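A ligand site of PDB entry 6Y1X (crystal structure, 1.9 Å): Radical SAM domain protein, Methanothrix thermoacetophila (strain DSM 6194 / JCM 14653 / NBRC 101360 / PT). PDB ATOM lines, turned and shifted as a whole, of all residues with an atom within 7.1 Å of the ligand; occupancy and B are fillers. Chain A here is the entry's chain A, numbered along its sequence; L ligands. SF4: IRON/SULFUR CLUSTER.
FE1 of the ligand is bound by OE2 of Glu 75 (2.2 Å).
FE3 of the ligand is bound by NE2 of His 52, 2.3 Å away.
FE2 of the ligand is bound by SG of Cys 39, 2.3 Å away.
An iron atom (FE4) of the ligand is bound by the side-chain sulfur (SG) of Cys 138 (2.3 Å).
A sulfur (S3) of the ligand sits close to the side-chain hydroxyl (OG1) of Thr 162.
The guanidinium group (NH1) of Arg 50 sits close to a sulfur (S4) of the ligand (3.5 Å).
S3 of the ligand sits close to NZ of Lys 215 (3.7 Å).
The side-chain amino group of Lys 215 lies close to the side-chain carboxylate of Glu 75 (3.0 Å).
The backbone NH (N) of Cys 39 is in hydrogen-bond range of a ring nitrogen (ND1) of His 37, at 3.1 Å.
A ring nitrogen (NE2) of His 37 sits close to the side-chain sulfur (SG) of Cys 138, 3.3 Å away.
The backbone carbonyl oxygen (O) of Asn 160 sits close to the side-chain sulfur (SG) of Cys 138, 3.7 Å away.
OG1 of Thr 162 is in hydrogen-bond range of NZ of Lys 215 (3.0 Å).
The backbone NH (N) of Ala 108 lies within hydrogen-bond range of the backbone carbonyl oxygen (O) of Met 51.
NZ of Lys 215 is in hydrogen-bond range of OD1 of Asn 217 (3.1 Å).
The backbone NH (N) of Lys 215 lies within hydrogen-bond range of the backbone carbonyl oxygen (O) of Ile 161, at 2.8 Å.
Merely in contact with the ligand: His 37, Ala 108, Phe 40, Ser 140, Val 106 and Ala 110.
Hydrophobic or aromatic side chains that line the ligand: His 37, Phe 40, His 52, Val 106, Ala 108 and Ala 110.
Of the 26 residues printed, 13 come within 4 Å of the ligand.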
ATOM      1  N   HIS A  37      29.433  -5.648   1.769  1.00  0.00           N
ATOM      2  CA  HIS A  37      28.180  -6.328   1.485  1.00  0.00           C
ATOM      3  C   HIS A  37      28.469  -7.458   0.509  1.00  0.00           C
ATOM      4  O   HIS A  37      28.881  -7.191  -0.626  1.00  0.00           O
ATOM      5  CB  HIS A  37      27.161  -5.360   0.905  1.00  0.00           C
ATOM      6  CG  HIS A  37      25.752  -5.882   0.876  1.00  0.00           C
ATOM      7  ND1 HIS A  37      25.436  -7.165   0.494  1.00  0.00           N
ATOM      8  CD2 HIS A  37      24.576  -5.280   1.186  1.00  0.00           C
ATOM      9  CE1 HIS A  37      24.134  -7.336   0.573  1.00  0.00           C
ATOM     10  NE2 HIS A  37      23.589  -6.213   0.985  1.00  0.00           N
ATOM     11  N   PRO A  38      28.256  -8.724   0.898  1.00  0.00           N
ATOM     12  CA  PRO A  38      28.623  -9.837   0.000  1.00  0.00           C
ATOM     13  C   PRO A  38      27.895  -9.823  -1.334  1.00  0.00           C
ATOM     14  O   PRO A  38      28.428 -10.348  -2.323  1.00  0.00           O
ATOM     15  CB  PRO A  38      28.281 -11.090   0.820  1.00  0.00           C
ATOM     16  CG  PRO A  38      27.987 -10.617   2.207  1.00  0.00           C
ATOM     17  CD  PRO A  38      27.622  -9.183   2.140  1.00  0.00           C
ATOM     18  N   CYS A  39      26.700  -9.244  -1.393  1.00  0.00           N
ATOM     19  CA  CYS A  39      25.915  -9.235  -2.623  1.00  0.00           C
ATOM     20  C   CYS A  39      26.210  -8.043  -3.521  1.00  0.00           C
ATOM     21  O   CYS A  39      25.756  -8.024  -4.661  1.00  0.00           O
ATOM     22  CB  CYS A  39      24.419  -9.281  -2.297  1.00  0.00           C
ATOM     23  SG  CYS A  39      23.972 -10.542  -1.073  1.00  0.00           S
ATOM     24  N   PHE A  40      26.983  -7.068  -3.034  1.00  0.00           N
ATOM     25  CA  PHE A  40      27.308  -5.893  -3.822  1.00  0.00           C
ATOM     26  C   PHE A  40      28.799  -5.791  -4.152  1.00  0.00           C
ATOM     27  O   PHE A  40      29.196  -4.876  -4.880  1.00  0.00           O
ATOM     28  CB  PHE A  40      26.854  -4.612  -3.108  1.00  0.00           C
ATOM     29  CG  PHE A  40      25.360  -4.458  -3.039  1.00  0.00           C
ATOM     30  CD1 PHE A  40      24.596  -5.257  -2.208  1.00  0.00           C
ATOM     31  CD2 PHE A  40      24.716  -3.513  -3.824  1.00  0.00           C
ATOM     32  CE1 PHE A  40      23.221  -5.117  -2.149  1.00  0.00           C
ATOM     33  CE2 PHE A  40      23.339  -3.359  -3.768  1.00  0.00           C
ATOM     34  CZ  PHE A  40      22.594  -4.169  -2.938  1.00  0.00           C
ATOM     35  N   ARG A  50      25.914 -12.652   5.439  1.00  0.00           N
ATOM     36  CA  ARG A  50      24.629 -11.995   5.571  1.00  0.00           C
ATOM     37  C   ARG A  50      23.650 -12.969   6.216  1.00  0.00           C
ATOM     38  O   ARG A  50      23.834 -14.188   6.173  1.00  0.00           O
ATOM     39  CB  ARG A  50      24.082 -11.537   4.220  1.00  0.00           C
ATOM     40  CG  ARG A  50      24.633 -12.323   3.037  1.00  0.00           C
ATOM     41  CD  ARG A  50      23.547 -12.711   2.044  1.00  0.00           C
ATOM     42  NE  ARG A  50      22.554 -13.604   2.627  1.00  0.00           N
ATOM     43  CZ  ARG A  50      21.790 -14.431   1.911  1.00  0.00           C
ATOM     44  NH1 ARG A  50      21.923 -14.490   0.596  1.00  0.00           N
ATOM     45  NH2 ARG A  50      20.909 -15.208   2.526  1.00  0.00           N
ATOM     46  N   MET A  51      22.595 -12.420   6.806  1.00  0.00           N
ATOM     47  CA  MET A  51      21.509 -13.230   7.346  1.00  0.00           C
ATOM     48  C   MET A  51      20.184 -12.628   6.938  1.00  0.00           C
ATOM     49  O   MET A  51      20.042 -11.408   6.864  1.00  0.00           O
ATOM     50  CB  MET A  51      21.618 -13.374   8.881  1.00  0.00           C
ATOM     51  CG  MET A  51      21.664 -12.065   9.642  1.00  0.00           C
ATOM     52  SD  MET A  51      21.790 -12.356  11.423  1.00  0.00           S
ATOM     53  CE  MET A  51      20.279 -13.246  11.759  1.00  0.00           C
ATOM     54  N   HIS A  52      19.215 -13.505   6.667  1.00  0.00           N
ATOM     55  CA  HIS A  52      17.864 -13.108   6.322  1.00  0.00           C
ATOM     56  C   HIS A  52      16.944 -13.325   7.520  1.00  0.00           C
ATOM     57  O   HIS A  52      17.051 -14.337   8.209  1.00  0.00           O
ATOM     58  CB  HIS A  52      17.343 -13.905   5.130  1.00  0.00           C
ATOM     59  CG  HIS A  52      17.900 -13.462   3.810  1.00  0.00           C
ATOM     60  ND1 HIS A  52      17.532 -14.039   2.613  1.00  0.00           N
ATOM     61  CD2 HIS A  52      18.813 -12.516   3.507  1.00  0.00           C
ATOM     62  CE1 HIS A  52      18.183 -13.454   1.628  1.00  0.00           C
ATOM     63  NE2 HIS A  52      18.977 -12.534   2.145  1.00  0.00           N
ATOM     64  N   ASN A  74      12.840 -14.967  -5.867  1.00  0.00           N
ATOM     65  CA  ASN A  74      13.684 -13.912  -6.408  1.00  0.00           C
ATOM     66  C   ASN A  74      14.943 -13.728  -5.582  1.00  0.00           C
ATOM     67  O   ASN A  74      15.990 -13.337  -6.124  1.00  0.00           O
ATOM     68  CB  ASN A  74      12.923 -12.581  -6.479  1.00  0.00           C
ATOM     69  CG  ASN A  74      11.794 -12.605  -7.484  1.00  0.00           C
ATOM     70  OD1 ASN A  74      11.816 -13.379  -8.435  1.00  0.00           O
ATOM     71  ND2 ASN A  74      10.803 -11.749  -7.269  1.00  0.00           N
ATOM     72  N   GLU A  75      14.877 -14.026  -4.283  1.00  0.00           N
ATOM     73  CA  GLU A  75      16.003 -13.752  -3.389  1.00  0.00           C
ATOM     74  C   GLU A  75      16.352 -14.964  -2.540  1.00  0.00           C
ATOM     75  O   GLU A  75      17.052 -14.827  -1.532  1.00  0.00           O
ATOM     76  CB  GLU A  75      15.712 -12.531  -2.505  1.00  0.00           C
ATOM     77  CG  GLU A  75      16.949 -11.686  -2.226  1.00  0.00           C
ATOM     78  CD  GLU A  75      17.410 -10.913  -3.448  1.00  0.00           C
ATOM     79  OE1 GLU A  75      16.825 -11.088  -4.541  1.00  0.00           O
ATOM     80  OE2 GLU A  75      18.374 -10.127  -3.342  1.00  0.00           O
ATOM     81  N   SER A  76      15.909 -16.150  -2.937  1.00  0.00           N
ATOM     82  CA  SER A  76      16.173 -17.369  -2.192  1.00  0.00           C
ATOM     83  C   SER A  76      16.388 -18.512  -3.162  1.00  0.00           C
ATOM     84  O   SER A  76      15.854 -18.511  -4.273  1.00  0.00           O
ATOM     85  CB  SER A  76      15.006 -17.722  -1.251  1.00  0.00           C
ATOM     86  OG  SER A  76      15.212 -18.957  -0.604  1.00  0.00           O
ATOM     87  N   VAL A 106      25.715  -7.926   7.274  1.00  0.00           N
ATOM     88  CA  VAL A 106      24.454  -7.491   6.690  1.00  0.00           C
ATOM     89  C   VAL A 106      23.311  -8.254   7.343  1.00  0.00           C
ATOM     90  O   VAL A 106      23.403  -9.459   7.578  1.00  0.00           O
ATOM     91  CB  VAL A 106      24.433  -7.705   5.150  1.00  0.00           C
ATOM     92  CG1 VAL A 106      23.092  -7.277   4.576  1.00  0.00           C
ATOM     93  CG2 VAL A 106      25.570  -6.944   4.490  1.00  0.00           C
ATOM     94  N   VAL A 107      22.223  -7.537   7.621  1.00  0.00           N
ATOM     95  CA  VAL A 107      20.957  -8.121   8.033  1.00  0.00           C
ATOM     96  C   VAL A 107      19.890  -7.649   7.064  1.00  0.00           C
ATOM     97  O   VAL A 107      19.783  -6.456   6.774  1.00  0.00           O
ATOM     98  CB  VAL A 107      20.605  -7.735   9.482  1.00  0.00           C
ATOM     99  CG1 VAL A 107      19.184  -8.125   9.810  1.00  0.00           C
ATOM    100  CG2 VAL A 107      21.566  -8.406  10.444  1.00  0.00           C
ATOM    101  N   ALA A 108      19.085  -8.589   6.566  1.00  0.00           N
ATOM    102  CA  ALA A 108      18.165  -8.271   5.481  1.00  0.00           C
ATOM    103  C   ALA A 108      16.827  -8.938   5.732  1.00  0.00           C
ATOM    104  O   ALA A 108      16.728  -9.935   6.446  1.00  0.00           O
ATOM    105  CB  ALA A 108      18.714  -8.711   4.120  1.00  0.00           C
ATOM    106  N   VAL A 109      15.797  -8.356   5.139  1.00  0.00           N
ATOM    107  CA  VAL A 109      14.493  -8.999   5.024  1.00  0.00           C
ATOM    108  C   VAL A 109      14.245  -9.209   3.548  1.00  0.00           C
ATOM    109  O   VAL A 109      14.289  -8.252   2.760  1.00  0.00           O
ATOM    110  CB  VAL A 109      13.382  -8.169   5.679  1.00  0.00           C
ATOM    111  CG1 VAL A 109      12.025  -8.857   5.501  1.00  0.00           C
ATOM    112  CG2 VAL A 109      13.691  -7.932   7.156  1.00  0.00           C
ATOM    113  N   ALA A 110      13.987 -10.451   3.165  1.00  0.00           N
ATOM    114  CA  ALA A 110      13.832 -10.819   1.761  1.00  0.00           C
ATOM    115  C   ALA A 110      12.686 -11.788   1.542  1.00  0.00           C
ATOM    116  O   ALA A 110      12.466 -12.214   0.402  1.00  0.00           O
ATOM    117  CB  ALA A 110      15.140 -11.440   1.224  1.00  0.00           C
ATOM    118  N   LEU A 137      21.811  -2.587   6.730  1.00  0.00           N
ATOM    119  CA  LEU A 137      20.424  -3.003   6.624  1.00  0.00           C
ATOM    120  C   LEU A 137      20.018  -3.009   5.152  1.00  0.00           C
ATOM    121  O   LEU A 137      20.240  -2.040   4.430  1.00  0.00           O
ATOM    122  CB  LEU A 137      19.501  -2.073   7.417  1.00  0.00           C
ATOM    123  CG  LEU A 137      19.792  -1.952   8.915  1.00  0.00           C
ATOM    124  CD1 LEU A 137      18.810  -0.993   9.579  1.00  0.00           C
ATOM    125  CD2 LEU A 137      19.759  -3.316   9.602  1.00  0.00           C
ATOM    126  N   CYS A 138      19.448  -4.138   4.727  1.00  0.00           N
ATOM    127  CA  CYS A 138      19.206  -4.443   3.327  1.00  0.00           C
ATOM    128  C   CYS A 138      17.799  -4.993   3.190  1.00  0.00           C
ATOM    129  O   CYS A 138      17.276  -5.631   4.113  1.00  0.00           O
ATOM    130  CB  CYS A 138      20.242  -5.459   2.806  1.00  0.00           C
ATOM    131  SG  CYS A 138      20.289  -5.767   1.015  1.00  0.00           S
ATOM    132  N   ILE A 139      17.164  -4.722   2.060  1.00  0.00           N
ATOM    133  CA  ILE A 139      15.871  -5.305   1.748  1.00  0.00           C
ATOM    134  C   ILE A 139      15.823  -5.672   0.280  1.00  0.00           C
ATOM    135  O   ILE A 139      16.463  -5.040  -0.566  1.00  0.00           O
ATOM    136  CB  ILE A 139      14.673  -4.376   2.097  1.00  0.00           C
ATOM    137  CG1 ILE A 139      14.672  -3.103   1.244  1.00  0.00           C
ATOM    138  CG2 ILE A 139      14.641  -4.026   3.563  1.00  0.00           C
ATOM    139  CD1 ILE A 139      13.639  -3.122   0.126  1.00  0.00           C
ATOM    140  N   SER A 140      15.022  -6.690  -0.015  1.00  0.00           N
ATOM    141  CA  SER A 140      14.649  -7.085  -1.366  1.00  0.00           C
ATOM    142  C   SER A 140      13.178  -6.763  -1.562  1.00  0.00           C
ATOM    143  O   SER A 140      12.399  -6.787  -0.611  1.00  0.00           O
ATOM    144  CB  SER A 140      14.917  -8.586  -1.587  1.00  0.00           C
ATOM    145  OG  SER A 140      14.337  -9.066  -2.786  1.00  0.00           O
ATOM    146  N   THR A 141      12.799  -6.423  -2.786  1.00  0.00           N
ATOM    147  CA  THR A 141      11.408  -6.101  -3.061  1.00  0.00           C
ATOM    148  C   THR A 141      11.096  -6.380  -4.521  1.00  0.00           C
ATOM    149  O   THR A 141      11.977  -6.326  -5.380  1.00  0.00           O
ATOM    150  CB  THR A 141      11.082  -4.636  -2.739  1.00  0.00           C
ATOM    151  OG1 THR A 141       9.702  -4.347  -3.043  1.00  0.00           O
ATOM    152  CG2 THR A 141      11.973  -3.685  -3.522  1.00  0.00           C
ATOM    153  N   ASN A 160      20.730  -0.365   1.355  1.00  0.00           N
ATOM    154  CA  ASN A 160      20.894  -1.211   0.187  1.00  0.00           C
ATOM    155  C   ASN A 160      19.540  -1.822  -0.127  1.00  0.00           C
ATOM    156  O   ASN A 160      18.867  -2.325   0.776  1.00  0.00           O
ATOM    157  CB  ASN A 160      21.925  -2.323   0.429  1.00  0.00           C
ATOM    158  CG  ASN A 160      23.335  -1.780   0.639  1.00  0.00           C
ATOM    159  OD1 ASN A 160      23.606  -1.108   1.631  1.00  0.00           O
ATOM    160  ND2 ASN A 160      24.219  -2.084  -0.289  1.00  0.00           N
ATOM    161  N   ILE A 161      19.157  -1.799  -1.397  1.00  0.00           N
ATOM    162  CA  ILE A 161      17.831  -2.235  -1.822  1.00  0.00           C
ATOM    163  C   ILE A 161      17.978  -3.079  -3.077  1.00  0.00           C
ATOM    164  O   ILE A 161      18.674  -2.682  -4.019  1.00  0.00           O
ATOM    165  CB  ILE A 161      16.883  -1.045  -2.090  1.00  0.00           C
ATOM    166  CG1 ILE A 161      16.595  -0.280  -0.796  1.00  0.00           C
ATOM    167  CG2 ILE A 161      15.581  -1.529  -2.711  1.00  0.00           C
ATOM    168  CD1 ILE A 161      15.791   0.980  -1.001  1.00  0.00           C
ATOM    169  N   THR A 162      17.358  -4.247  -3.083  1.00  0.00           N
ATOM    170  CA  THR A 162      17.287  -5.065  -4.276  1.00  0.00           C
ATOM    171  C   THR A 162      15.866  -5.012  -4.813  1.00  0.00           C
ATOM    172  O   THR A 162      14.909  -5.260  -4.080  1.00  0.00           O
ATOM    173  CB  THR A 162      17.665  -6.514  -3.967  1.00  0.00           C
ATOM    174  OG1 THR A 162      19.081  -6.598  -3.736  1.00  0.00           O
ATOM    175  CG2 THR A 162      17.310  -7.421  -5.135  1.00  0.00           C
ATOM    176  N   LYS A 215      20.485  -2.679  -6.217  1.00  0.00           N
ATOM    177  CA  LYS A 215      20.763  -3.846  -7.034  1.00  0.00           C
ATOM    178  C   LYS A 215      19.480  -4.273  -7.726  1.00  0.00           C
ATOM    179  O   LYS A 215      18.410  -4.286  -7.105  1.00  0.00           O
ATOM    180  CB  LYS A 215      21.328  -4.982  -6.169  1.00  0.00           C
ATOM    181  CG  LYS A 215      21.229  -6.377  -6.754  1.00  0.00           C
ATOM    182  CD  LYS A 215      22.120  -7.321  -5.952  1.00  0.00           C
ATOM    183  CE  LYS A 215      21.618  -8.754  -5.972  1.00  0.00           C
ATOM    184  NZ  LYS A 215      20.392  -8.921  -5.148  1.00  0.00           N
ATOM    185  N   ASN A 217      17.682  -7.402  -9.673  1.00  0.00           N
ATOM    186  CA  ASN A 217      17.625  -8.786 -10.128  1.00  0.00           C
ATOM    187  C   ASN A 217      16.759  -8.877 -11.370  1.00  0.00           C
ATOM    188  O   ASN A 217      15.724  -8.209 -11.478  1.00  0.00           O
ATOM    189  CB  ASN A 217      17.013  -9.692  -9.056  1.00  0.00           C
ATOM    190  CG  ASN A 217      17.889  -9.822  -7.825  1.00  0.00           C
ATOM    191  OD1 ASN A 217      19.085  -9.558  -7.850  1.00  0.00           O
ATOM    192  ND2 ASN A 217      17.272 -10.270  -6.736  1.00  0.00           N
ATOM    193  N   MET A 280      26.474  -8.850 -11.226  1.00  0.00           N
ATOM    194  CA  MET A 280      26.784  -9.670 -10.053  1.00  0.00           C
ATOM    195  C   MET A 280      27.088 -11.093 -10.517  1.00  0.00           C
ATOM    196  O   MET A 280      26.247 -11.712 -11.179  1.00  0.00           O
ATOM    197  CB  MET A 280      25.631  -9.651  -9.066  1.00  0.00           C
ATOM    198  CG  MET A 280      25.938 -10.338  -7.737  1.00  0.00           C
ATOM    199  SD  MET A 280      24.446 -10.765  -6.809  1.00  0.00           S
ATOM    200  CE  MET A 280      25.127 -11.685  -5.438  1.00  0.00           C
HETATM  201 FE1  SF4 L   1      19.361  -9.699  -1.429  1.00  0.00          FE
HETATM  202 FE2  SF4 L   1      21.854  -9.987  -0.375  1.00  0.00          FE
HETATM  203 FE3  SF4 L   1      19.652 -10.678   1.061  1.00  0.00          FE
HETATM  204 FE4  SF4 L   1      20.205  -8.026   0.579  1.00  0.00          FE
HETATM  205  S1  SF4 L   1      21.461  -9.477   1.831  1.00  0.00           S
HETATM  206  S2  SF4 L   1      18.152  -9.054   0.425  1.00  0.00           S
HETATM  207  S3  SF4 L   1      21.072  -8.167  -1.542  1.00  0.00           S
HETATM  208  S4  SF4 L   1      20.381 -11.685  -0.874  1.00  0.00           S
